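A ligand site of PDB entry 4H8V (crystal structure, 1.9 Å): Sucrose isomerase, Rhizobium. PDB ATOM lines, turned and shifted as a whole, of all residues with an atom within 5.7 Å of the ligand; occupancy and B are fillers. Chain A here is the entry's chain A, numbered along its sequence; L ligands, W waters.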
ATOM      1  N   ASP A  61     -26.767  -7.946  21.146  1.00  0.00           N
ATOM      2  CA  ASP A  61     -26.588  -7.980  19.712  1.00  0.00           C
ATOM      3  C   ASP A  61     -26.438  -6.536  19.219  1.00  0.00           C
ATOM      4  O   ASP A  61     -26.939  -6.170  18.152  1.00  0.00           O
ATOM      5  CB  ASP A  61     -27.784  -8.664  19.047  1.00  0.00           C
ATOM      6  CG  ASP A  61     -27.552  -8.955  17.579  1.00  0.00           C
ATOM      7  OD1 ASP A  61     -26.387  -8.913  17.145  1.00  0.00           O
ATOM      8  OD2 ASP A  61     -28.548  -9.239  16.863  1.00  0.00           O
ATOM      9  N   TYR A  64     -29.721  -4.513  18.169  1.00  0.00           N
ATOM     10  CA  TYR A  64     -30.801  -5.245  17.531  1.00  0.00           C
ATOM     11  C   TYR A  64     -31.642  -6.079  18.520  1.00  0.00           C
ATOM     12  O   TYR A  64     -32.474  -6.887  18.121  1.00  0.00           O
ATOM     13  CB  TYR A  64     -30.256  -6.092  16.382  1.00  0.00           C
ATOM     14  CG  TYR A  64     -29.799  -5.278  15.192  1.00  0.00           C
ATOM     15  CD1 TYR A  64     -30.707  -4.870  14.224  1.00  0.00           C
ATOM     16  CD2 TYR A  64     -28.451  -4.936  15.023  1.00  0.00           C
ATOM     17  CE1 TYR A  64     -30.292  -4.127  13.121  1.00  0.00           C
ATOM     18  CE2 TYR A  64     -28.032  -4.194  13.928  1.00  0.00           C
ATOM     19  CZ  TYR A  64     -28.958  -3.810  12.976  1.00  0.00           C
ATOM     20  OH  TYR A  64     -28.559  -3.068  11.891  1.00  0.00           O
ATOM     21  N   VAL A 101     -36.300  -2.440  13.790  1.00  0.00           N
ATOM     22  CA  VAL A 101     -36.065  -3.836  14.163  1.00  0.00           C
ATOM     23  C   VAL A 101     -37.310  -4.403  14.851  1.00  0.00           C
ATOM     24  O   VAL A 101     -37.429  -4.351  16.080  1.00  0.00           O
ATOM     25  CB  VAL A 101     -34.892  -3.906  15.140  1.00  0.00           C
ATOM     26  CG1 VAL A 101     -34.471  -5.352  15.394  1.00  0.00           C
ATOM     27  CG2 VAL A 101     -33.742  -3.094  14.605  1.00  0.00           C
ATOM     28  N   HIS A 104     -38.372  -8.915  15.996  1.00  0.00           N
ATOM     29  CA  HIS A 104     -38.157  -9.437  17.329  1.00  0.00           C
ATOM     30  C   HIS A 104     -37.847  -8.254  18.240  1.00  0.00           C
ATOM     31  O   HIS A 104     -37.456  -7.197  17.770  1.00  0.00           O
ATOM     32  CB  HIS A 104     -36.991 -10.458  17.334  1.00  0.00           C
ATOM     33  CG  HIS A 104     -35.749  -9.955  16.660  1.00  0.00           C
ATOM     34  ND1 HIS A 104     -35.478 -10.199  15.327  1.00  0.00           N
ATOM     35  CD2 HIS A 104     -34.734  -9.204  17.120  1.00  0.00           C
ATOM     36  CE1 HIS A 104     -34.341  -9.623  15.005  1.00  0.00           C
ATOM     37  NE2 HIS A 104     -33.866  -9.001  16.070  1.00  0.00           N
ATOM     38  N   PHE A 144     -30.211 -18.614  14.086  1.00  0.00           N
ATOM     39  CA  PHE A 144     -29.072 -17.988  13.424  1.00  0.00           C
ATOM     40  C   PHE A 144     -27.854 -17.905  14.349  1.00  0.00           C
ATOM     41  O   PHE A 144     -26.726 -17.981  13.901  1.00  0.00           O
ATOM     42  CB  PHE A 144     -29.424 -16.575  12.941  1.00  0.00           C
ATOM     43  CG  PHE A 144     -30.254 -16.550  11.683  1.00  0.00           C
ATOM     44  CD1 PHE A 144     -29.667 -16.691  10.441  1.00  0.00           C
ATOM     45  CD2 PHE A 144     -31.634 -16.339  11.758  1.00  0.00           C
ATOM     46  CE1 PHE A 144     -30.429 -16.648   9.287  1.00  0.00           C
ATOM     47  CE2 PHE A 144     -32.405 -16.314  10.605  1.00  0.00           C
ATOM     48  CZ  PHE A 144     -31.818 -16.465   9.373  1.00  0.00           C
ATOM     49  N   PHE A 145     -28.089 -17.718  15.644  1.00  0.00           N
ATOM     50  CA  PHE A 145     -27.003 -17.530  16.593  1.00  0.00           C
ATOM     51  C   PHE A 145     -26.756 -18.753  17.470  1.00  0.00           C
ATOM     52  O   PHE A 145     -26.259 -18.637  18.585  1.00  0.00           O
ATOM     53  CB  PHE A 145     -27.244 -16.289  17.449  1.00  0.00           C
ATOM     54  CG  PHE A 145     -27.285 -15.019  16.661  1.00  0.00           C
ATOM     55  CD1 PHE A 145     -26.736 -14.962  15.380  1.00  0.00           C
ATOM     56  CD2 PHE A 145     -27.881 -13.880  17.177  1.00  0.00           C
ATOM     57  CE1 PHE A 145     -26.778 -13.790  14.643  1.00  0.00           C
ATOM     58  CE2 PHE A 145     -27.920 -12.709  16.449  1.00  0.00           C
ATOM     59  CZ  PHE A 145     -27.363 -12.667  15.173  1.00  0.00           C
ATOM     60  N   PHE A 164     -33.223 -15.477  16.113  1.00  0.00           N
ATOM     61  CA  PHE A 164     -31.887 -14.998  16.420  1.00  0.00           C
ATOM     62  C   PHE A 164     -31.501 -15.341  17.848  1.00  0.00           C
ATOM     63  O   PHE A 164     -31.658 -16.492  18.280  1.00  0.00           O
ATOM     64  CB  PHE A 164     -31.797 -13.483  16.136  1.00  0.00           C
ATOM     65  CG  PHE A 164     -32.003 -13.145  14.689  1.00  0.00           C
ATOM     66  CD1 PHE A 164     -33.267 -12.862  14.194  1.00  0.00           C
ATOM     67  CD2 PHE A 164     -30.927 -13.163  13.795  1.00  0.00           C
ATOM     68  CE1 PHE A 164     -33.465 -12.586  12.868  1.00  0.00           C
ATOM     69  CE2 PHE A 164     -31.131 -12.887  12.437  1.00  0.00           C
ATOM     70  CZ  PHE A 164     -32.393 -12.590  11.977  1.00  0.00           C
ATOM     71  N   GLN A 168     -33.668 -12.485  21.958  1.00  0.00           N
ATOM     72  CA  GLN A 168     -34.412 -11.785  20.916  1.00  0.00           C
ATOM     73  C   GLN A 168     -35.642 -12.590  20.494  1.00  0.00           C
ATOM     74  O   GLN A 168     -35.679 -13.138  19.402  1.00  0.00           O
ATOM     75  CB  GLN A 168     -33.500 -11.528  19.708  1.00  0.00           C
ATOM     76  CG  GLN A 168     -32.432 -10.504  19.964  1.00  0.00           C
ATOM     77  CD  GLN A 168     -31.326 -10.540  18.918  1.00  0.00           C
ATOM     78  OE1 GLN A 168     -30.818 -11.595  18.569  1.00  0.00           O
ATOM     79  NE2 GLN A 168     -30.961  -9.370  18.401  1.00  0.00           N
ATOM     80  N   ARG A 198     -34.908   1.738   7.374  1.00  0.00           N
ATOM     81  CA  ARG A 198     -34.443   0.485   6.834  1.00  0.00           C
ATOM     82  C   ARG A 198     -35.046  -0.598   7.702  1.00  0.00           C
ATOM     83  O   ARG A 198     -34.970  -0.513   8.922  1.00  0.00           O
ATOM     84  CB  ARG A 198     -32.910   0.443   6.904  1.00  0.00           C
ATOM     85  CG  ARG A 198     -32.269  -0.870   6.484  1.00  0.00           C
ATOM     86  CD  ARG A 198     -31.854  -1.666   7.699  1.00  0.00           C
ATOM     87  NE  ARG A 198     -30.947  -2.760   7.367  1.00  0.00           N
ATOM     88  CZ  ARG A 198     -30.587  -3.704   8.227  1.00  0.00           C
ATOM     89  NH1 ARG A 198     -31.034  -3.670   9.463  1.00  0.00           N
ATOM     90  NH2 ARG A 198     -29.752  -4.673   7.849  1.00  0.00           N
ATOM     91  N   ASP A 200     -34.932  -4.089   9.207  1.00  0.00           N
ATOM     92  CA  ASP A 200     -34.212  -5.293   9.628  1.00  0.00           C
ATOM     93  C   ASP A 200     -34.952  -6.607   9.314  1.00  0.00           C
ATOM     94  O   ASP A 200     -36.093  -6.776   9.739  1.00  0.00           O
ATOM     95  CB  ASP A 200     -34.010  -5.205  11.136  1.00  0.00           C
ATOM     96  CG  ASP A 200     -32.991  -6.186  11.632  1.00  0.00           C
ATOM     97  OD1 ASP A 200     -31.832  -6.050  11.205  1.00  0.00           O
ATOM     98  OD2 ASP A 200     -33.341  -7.077  12.457  1.00  0.00           O
ATOM     99  N   THR A 201     -34.263  -7.549   8.630  1.00  0.00           N
ATOM    100  CA  THR A 201     -34.833  -8.848   8.215  1.00  0.00           C
ATOM    101  C   THR A 201     -36.353  -8.772   7.953  1.00  0.00           C
ATOM    102  O   THR A 201     -37.146  -9.420   8.636  1.00  0.00           O
ATOM    103  CB  THR A 201     -34.422 -10.059   9.185  1.00  0.00           C
ATOM    104  OG1 THR A 201     -35.028 -11.273   8.735  1.00  0.00           O
ATOM    105  CG2 THR A 201     -34.797  -9.829  10.643  1.00  0.00           C
ATOM    106  N   GLU A 254     -34.390  -4.805   4.220  1.00  0.00           N
ATOM    107  CA  GLU A 254     -33.322  -5.809   4.218  1.00  0.00           C
ATOM    108  C   GLU A 254     -33.952  -7.155   3.947  1.00  0.00           C
ATOM    109  O   GLU A 254     -34.467  -7.792   4.859  1.00  0.00           O
ATOM    110  CB  GLU A 254     -32.556  -5.862   5.547  1.00  0.00           C
ATOM    111  CG  GLU A 254     -31.382  -6.849   5.464  1.00  0.00           C
ATOM    112  CD  GLU A 254     -31.024  -7.505   6.775  1.00  0.00           C
ATOM    113  OE1 GLU A 254     -31.913  -7.680   7.627  1.00  0.00           O
ATOM    114  OE2 GLU A 254     -29.837  -7.889   6.942  1.00  0.00           O
ATOM    115  N   PHE A 256     -33.199 -10.375   3.638  1.00  0.00           N
ATOM    116  CA  PHE A 256     -32.258 -11.469   3.794  1.00  0.00           C
ATOM    117  C   PHE A 256     -32.906 -12.836   3.696  1.00  0.00           C
ATOM    118  O   PHE A 256     -33.858 -13.124   4.414  1.00  0.00           O
ATOM    119  CB  PHE A 256     -31.507 -11.356   5.112  1.00  0.00           C
ATOM    120  CG  PHE A 256     -30.288 -12.209   5.154  1.00  0.00           C
ATOM    121  CD1 PHE A 256     -29.070 -11.721   4.701  1.00  0.00           C
ATOM    122  CD2 PHE A 256     -30.352 -13.519   5.616  1.00  0.00           C
ATOM    123  CE1 PHE A 256     -27.934 -12.521   4.723  1.00  0.00           C
ATOM    124  CE2 PHE A 256     -29.233 -14.322   5.635  1.00  0.00           C
ATOM    125  CZ  PHE A 256     -28.013 -13.822   5.195  1.00  0.00           C
ATOM    126  N   PHE A 280     -28.925  -9.688  -0.930  1.00  0.00           N
ATOM    127  CA  PHE A 280     -27.676 -10.258  -0.442  1.00  0.00           C
ATOM    128  C   PHE A 280     -27.113 -11.290  -1.373  1.00  0.00           C
ATOM    129  O   PHE A 280     -26.119 -11.944  -1.046  1.00  0.00           O
ATOM    130  CB  PHE A 280     -27.848 -10.760   1.001  1.00  0.00           C
ATOM    131  CG  PHE A 280     -28.144  -9.643   1.930  1.00  0.00           C
ATOM    132  CD1 PHE A 280     -27.130  -8.987   2.598  1.00  0.00           C
ATOM    133  CD2 PHE A 280     -29.444  -9.164   2.056  1.00  0.00           C
ATOM    134  CE1 PHE A 280     -27.394  -7.917   3.427  1.00  0.00           C
ATOM    135  CE2 PHE A 280     -29.696  -8.091   2.857  1.00  0.00           C
ATOM    136  CZ  PHE A 280     -28.658  -7.458   3.544  1.00  0.00           C
ATOM    137  N   ARG A 284     -23.162 -12.149  -0.480  1.00  0.00           N
ATOM    138  CA  ARG A 284     -22.955 -13.550  -0.083  1.00  0.00           C
ATOM    139  C   ARG A 284     -22.740 -14.456  -1.298  1.00  0.00           C
ATOM    140  O   ARG A 284     -22.894 -15.681  -1.193  1.00  0.00           O
ATOM    141  CB  ARG A 284     -24.169 -14.065   0.744  1.00  0.00           C
ATOM    142  CG  ARG A 284     -24.418 -13.358   2.076  1.00  0.00           C
ATOM    143  CD  ARG A 284     -23.266 -13.542   3.043  1.00  0.00           C
ATOM    144  NE  ARG A 284     -23.384 -12.710   4.255  1.00  0.00           N
ATOM    145  CZ  ARG A 284     -23.930 -13.097   5.402  1.00  0.00           C
ATOM    146  NH1 ARG A 284     -24.431 -14.329   5.537  1.00  0.00           N
ATOM    147  NH2 ARG A 284     -23.958 -12.270   6.437  1.00  0.00           N
ATOM    148  N   ARG A 287     -20.358 -17.070  -0.377  1.00  0.00           N
ATOM    149  CA  ARG A 287     -20.508 -17.615   0.970  1.00  0.00           C
ATOM    150  C   ARG A 287     -21.173 -18.995   0.878  1.00  0.00           C
ATOM    151  O   ARG A 287     -22.160 -19.158   0.167  1.00  0.00           O
ATOM    152  CB  ARG A 287     -21.307 -16.658   1.832  1.00  0.00           C
ATOM    153  CG  ARG A 287     -21.264 -16.950   3.330  1.00  0.00           C
ATOM    154  CD  ARG A 287     -19.963 -16.517   3.959  1.00  0.00           C
ATOM    155  NE  ARG A 287     -19.783 -15.070   3.968  1.00  0.00           N
ATOM    156  CZ  ARG A 287     -20.187 -14.265   4.954  1.00  0.00           C
ATOM    157  NH1 ARG A 287     -20.808 -14.766   6.016  1.00  0.00           N
ATOM    158  NH2 ARG A 287     -19.986 -12.951   4.863  1.00  0.00           N
ATOM    159  N   ARG A 291     -22.849 -20.350   5.937  1.00  0.00           N
ATOM    160  CA  ARG A 291     -22.679 -18.921   6.217  1.00  0.00           C
ATOM    161  C   ARG A 291     -21.372 -18.554   6.899  1.00  0.00           C
ATOM    162  O   ARG A 291     -21.177 -17.411   7.287  1.00  0.00           O
ATOM    163  CB  ARG A 291     -23.881 -18.347   7.005  1.00  0.00           C
ATOM    164  CG  ARG A 291     -25.247 -18.825   6.511  1.00  0.00           C
ATOM    165  CD  ARG A 291     -26.417 -18.095   7.199  1.00  0.00           C
ATOM    166  NE  ARG A 291     -26.129 -17.701   8.571  1.00  0.00           N
ATOM    167  CZ  ARG A 291     -26.345 -18.449   9.647  1.00  0.00           C
ATOM    168  NH1 ARG A 291     -26.848 -19.668   9.516  1.00  0.00           N
ATOM    169  NH2 ARG A 291     -26.036 -17.978  10.843  1.00  0.00           N
ATOM    170  N   HIS A 326     -22.408  -3.800   8.256  1.00  0.00           N
ATOM    171  CA  HIS A 326     -22.004  -4.195   9.588  1.00  0.00           C
ATOM    172  C   HIS A 326     -22.161  -5.704   9.794  1.00  0.00           C
ATOM    173  O   HIS A 326     -21.858  -6.215  10.863  1.00  0.00           O
ATOM    174  CB  HIS A 326     -22.871  -3.482  10.622  1.00  0.00           C
ATOM    175  CG  HIS A 326     -24.321  -3.839  10.512  1.00  0.00           C
ATOM    176  ND1 HIS A 326     -25.080  -3.532   9.413  1.00  0.00           N
ATOM    177  CD2 HIS A 326     -25.143  -4.502  11.364  1.00  0.00           C
ATOM    178  CE1 HIS A 326     -26.313  -3.991   9.586  1.00  0.00           C
ATOM    179  NE2 HIS A 326     -26.372  -4.586  10.758  1.00  0.00           N
ATOM    180  N   ASP A 327     -22.636  -6.412   8.771  1.00  0.00           N
ATOM    181  CA  ASP A 327     -22.812  -7.861   8.906  1.00  0.00           C
ATOM    182  C   ASP A 327     -21.839  -8.651   8.022  1.00  0.00           C
ATOM    183  O   ASP A 327     -21.946  -9.883   7.925  1.00  0.00           O
ATOM    184  CB  ASP A 327     -24.251  -8.265   8.571  1.00  0.00           C
ATOM    185  CG  ASP A 327     -25.255  -7.774   9.610  1.00  0.00           C
ATOM    186  OD1 ASP A 327     -24.890  -7.562  10.781  1.00  0.00           O
ATOM    187  OD2 ASP A 327     -26.432  -7.594   9.236  1.00  0.00           O
ATOM    188  N   GLU A 386     -22.658 -14.145  16.791  1.00  0.00           N
ATOM    189  CA  GLU A 386     -22.776 -15.136  15.710  1.00  0.00           C
ATOM    190  C   GLU A 386     -21.586 -16.131  15.640  1.00  0.00           C
ATOM    191  O   GLU A 386     -21.758 -17.287  15.239  1.00  0.00           O
ATOM    192  CB  GLU A 386     -22.929 -14.457  14.350  1.00  0.00           C
ATOM    193  CG  GLU A 386     -23.293 -15.425  13.221  1.00  0.00           C
ATOM    194  CD  GLU A 386     -23.483 -14.748  11.867  1.00  0.00           C
ATOM    195  OE1 GLU A 386     -22.842 -13.713  11.611  1.00  0.00           O
ATOM    196  OE2 GLU A 386     -24.275 -15.261  11.061  1.00  0.00           O
ATOM    197  N   PHE A 390     -21.538 -20.277  15.815  1.00  0.00           N
ATOM    198  CA  PHE A 390     -20.783 -21.229  15.008  1.00  0.00           C
ATOM    199  C   PHE A 390     -19.976 -22.227  15.870  1.00  0.00           C
ATOM    200  O   PHE A 390     -19.914 -23.417  15.576  1.00  0.00           O
ATOM    201  CB  PHE A 390     -19.828 -20.486  14.062  1.00  0.00           C
ATOM    202  CG  PHE A 390     -20.519 -19.656  13.005  1.00  0.00           C
ATOM    203  CD1 PHE A 390     -21.659 -20.118  12.373  1.00  0.00           C
ATOM    204  CD2 PHE A 390     -20.035 -18.411  12.646  1.00  0.00           C
ATOM    205  CE1 PHE A 390     -22.299 -19.353  11.404  1.00  0.00           C
ATOM    206  CE2 PHE A 390     -20.671 -17.647  11.686  1.00  0.00           C
ATOM    207  CZ  PHE A 390     -21.799 -18.115  11.058  1.00  0.00           C
ATOM    208  N   ARG A 414     -18.580 -10.657  10.888  1.00  0.00           N
ATOM    209  CA  ARG A 414     -19.127  -9.305  10.869  1.00  0.00           C
ATOM    210  C   ARG A 414     -18.203  -8.348  11.595  1.00  0.00           C
ATOM    211  O   ARG A 414     -18.170  -7.146  11.276  1.00  0.00           O
ATOM    212  CB  ARG A 414     -20.484  -9.257  11.577  1.00  0.00           C
ATOM    213  CG  ARG A 414     -21.301 -10.504  11.444  1.00  0.00           C
ATOM    214  CD  ARG A 414     -22.737 -10.226  11.826  1.00  0.00           C
ATOM    215  NE  ARG A 414     -22.989 -10.301  13.265  1.00  0.00           N
ATOM    216  CZ  ARG A 414     -24.215 -10.294  13.769  1.00  0.00           C
ATOM    217  NH1 ARG A 414     -25.246 -10.195  12.943  1.00  0.00           N
ATOM    218  NH2 ARG A 414     -24.418 -10.372  15.073  1.00  0.00           N
ATOM    219  N   ARG A 418     -16.593  -3.947  12.153  1.00  0.00           N
ATOM    220  CA  ARG A 418     -17.011  -3.262  13.372  1.00  0.00           C
ATOM    221  C   ARG A 418     -15.851  -2.684  14.170  1.00  0.00           C
ATOM    222  O   ARG A 418     -16.060  -2.056  15.202  1.00  0.00           O
ATOM    223  CB  ARG A 418     -17.870  -4.198  14.251  1.00  0.00           C
ATOM    224  CG  ARG A 418     -19.189  -4.636  13.596  1.00  0.00           C
ATOM    225  CD  ARG A 418     -19.971  -5.677  14.377  1.00  0.00           C
ATOM    226  NE  ARG A 418     -21.159  -6.067  13.634  1.00  0.00           N
ATOM    227  CZ  ARG A 418     -22.220  -6.688  14.158  1.00  0.00           C
ATOM    228  NH1 ARG A 418     -22.253  -6.993  15.444  1.00  0.00           N
ATOM    229  NH2 ARG A 418     -23.251  -6.993  13.377  1.00  0.00           N
HETATM  230  O1  LIG L   1     -29.502  -9.375   9.817  1.00  0.00           O
HETATM  231  C1  LIG L   1     -30.314 -10.204   9.024  1.00  0.00           C
HETATM  232  C2  LIG L   1     -29.911 -11.678   8.981  1.00  0.00           C
HETATM  233  O2  LIG L   1     -30.681 -12.582   9.308  1.00  0.00           O
HETATM  234  C3  LIG L   1     -28.529 -12.088   8.570  1.00  0.00           C
HETATM  235  O3  LIG L   1     -27.836 -10.944   8.184  1.00  0.00           O
HETATM  236  C4  LIG L   1     -27.928 -12.801   9.778  1.00  0.00           C
HETATM  237  O4  LIG L   1     -28.022 -11.991  10.875  1.00  0.00           O
HETATM  238  C5  LIG L   1     -26.506 -13.211   9.617  1.00  0.00           C
HETATM  239  O5  LIG L   1     -25.723 -12.086   9.700  1.00  0.00           O
HETATM  240  C6  LIG L   1     -26.253 -13.863   8.303  1.00  0.00           C
HETATM  241  O6  LIG L   1     -25.282 -14.843   8.240  1.00  0.00           O
HETATM  242  C7  LIG L   1     -30.061  -8.347  10.599  1.00  0.00           C
HETATM  243  C8  LIG L   1     -29.063  -7.280  11.074  1.00  0.00           C
HETATM  244  O7  LIG L   1     -28.537  -6.489  10.027  1.00  0.00           O
HETATM  245  C9  LIG L   1     -28.040  -7.933  11.992  1.00  0.00           C
HETATM  246  O8  LIG L   1     -26.864  -7.029  12.311  1.00  0.00           O
HETATM  247  C10 LIG L   1     -28.695  -8.498  13.172  1.00  0.00           C
HETATM  248  O9  LIG L   1     -27.805  -9.298  13.937  1.00  0.00           O
HETATM  249  C11 LIG L   1     -29.912  -9.345  12.859  1.00  0.00           C
HETATM  250  O10 LIG L   1     -30.765  -8.870  11.697  1.00  0.00           O
HETATM  251  C12 LIG L   1     -30.736  -9.499  14.098  1.00  0.00           C
HETATM  252  O11 LIG L   1     -31.620  -8.479  14.362  1.00  0.00           O
HETATM  253  O   HOH W   1     -32.810 -13.045   8.272  1.00  0.00           O
HETATM  254  O   HOH W   2     -25.633  -9.951   5.881  1.00  0.00           O
HETATM  255  O   HOH W   3     -25.913  -6.877  14.683  1.00  0.00           O
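The side-chain carboxylate (OE2) of Glu 254 lies close to an oxygen (O1) of the ligand (3.3 Å).
Tyr 64 touches the ligand (CB to O11, 3.4 Å).
CZ of Phe 145 touches O9 of the ligand, 3.6 Å away.
Phe 164 touches the ligand.
Phe 256 touches the ligand (CZ to C6, 3.6 Å).
Arg 418 touches the ligand.
Hydrophobic or aromatic side chains that line the ligand: Tyr 64, His 104, Phe 145, Phe 164, Phe 256 and His 326.
Within 4 Å of the ligand: Asp 61, Tyr 64, His 104, Phe 145, Phe 164, Arg 198, Asp 200, Glu 254, Phe 256, Arg 284, Arg 291, His 326, Asp 327, Glu 386, Arg 414 and Arg 418.
The nearest printed residue that does not touch the ligand is Phe 144 (4.05 Å).
An oxygen (O8) of the ligand sits at hydrogen-bond distance from a ring nitrogen (NE2) of His 326.
The guanidinium group (NH2) of Arg 198 sits at hydrogen-bond distance from an oxygen (O7) of the ligand (3.1 Å).
The guanidinium group of Arg 414 sits at hydrogen-bond distance from an oxygen (O9) of the ligand (2.9 Å).
A ring nitrogen (NE2) of His 104 sits at hydrogen-bond distance from an oxygen (O11) of the ligand (2.9 Å).
OE2 of Glu 386 is in hydrogen-bond range of O6 of the ligand (3.0 Å).
The side-chain carboxylate of Asp 200 sits at hydrogen-bond distance from an oxygen (O11) of the ligand.
An oxygen (O6) of the ligand is in hydrogen-bond range of the guanidinium group of Arg 284 (2.9 Å).
The side-chain carboxylate (OD2) of Asp 61 sits at hydrogen-bond distance from an oxygen (O9) of the ligand, at 3.0 Å.
An oxygen (O7) of the ligand sits at hydrogen-bond distance from the side-chain carboxylate (OD2) of Asp 327, 2.5 Å away.
NE of Arg 291 is in hydrogen-bond range of O6 of the ligand, at 3.0 Å.
A ring nitrogen (NE2) of His 326 sits close to the side-chain carboxylate (OD1) of Asp 327 (3.3 Å).
The guanidinium group (NE) of Arg 414 lies within salt-bridge range of the side-chain carboxylate (OE1) of Glu 386 (3.8 Å).
A ring nitrogen (NE2) of His 326 sits at hydrogen-bond distance from the side-chain hydroxyl of Tyr 64, at 2.9 Å.
OE1 of Glu 254 is in hydrogen-bond range of N of Thr 201 (2.6 Å).
The backbone carbonyl oxygen of Arg 291 lies within hydrogen-bond range of the guanidinium group of Arg 287, 3.0 Å away.
OE2 of Glu 386 is in salt-bridge range of NH2 of Arg 291 (3.2 Å).
O of Asp 327 is in hydrogen-bond range of NH2 of Arg 284 (3.5 Å).
The guanidinium group of Arg 291 is in hydrogen-bond range of the backbone carbonyl oxygen of Phe 144.
Water W1 bridges an oxygen (O2) of the ligand and the side-chain hydroxyl (OG1) of Thr 201.
Water W3 lies within hydrogen-bond range of an oxygen (O8) of the ligand (2.6 Å), the guanidinium group (NH2) of Arg 418 (3.0 Å) and the side-chain carboxylate (OD1) of Asp 61 (3.2 Å).
Water W2 bridges the guanidinium group of Arg 284 (2.9 Å) and an oxygen (O3) of the ligand (3.3 Å).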
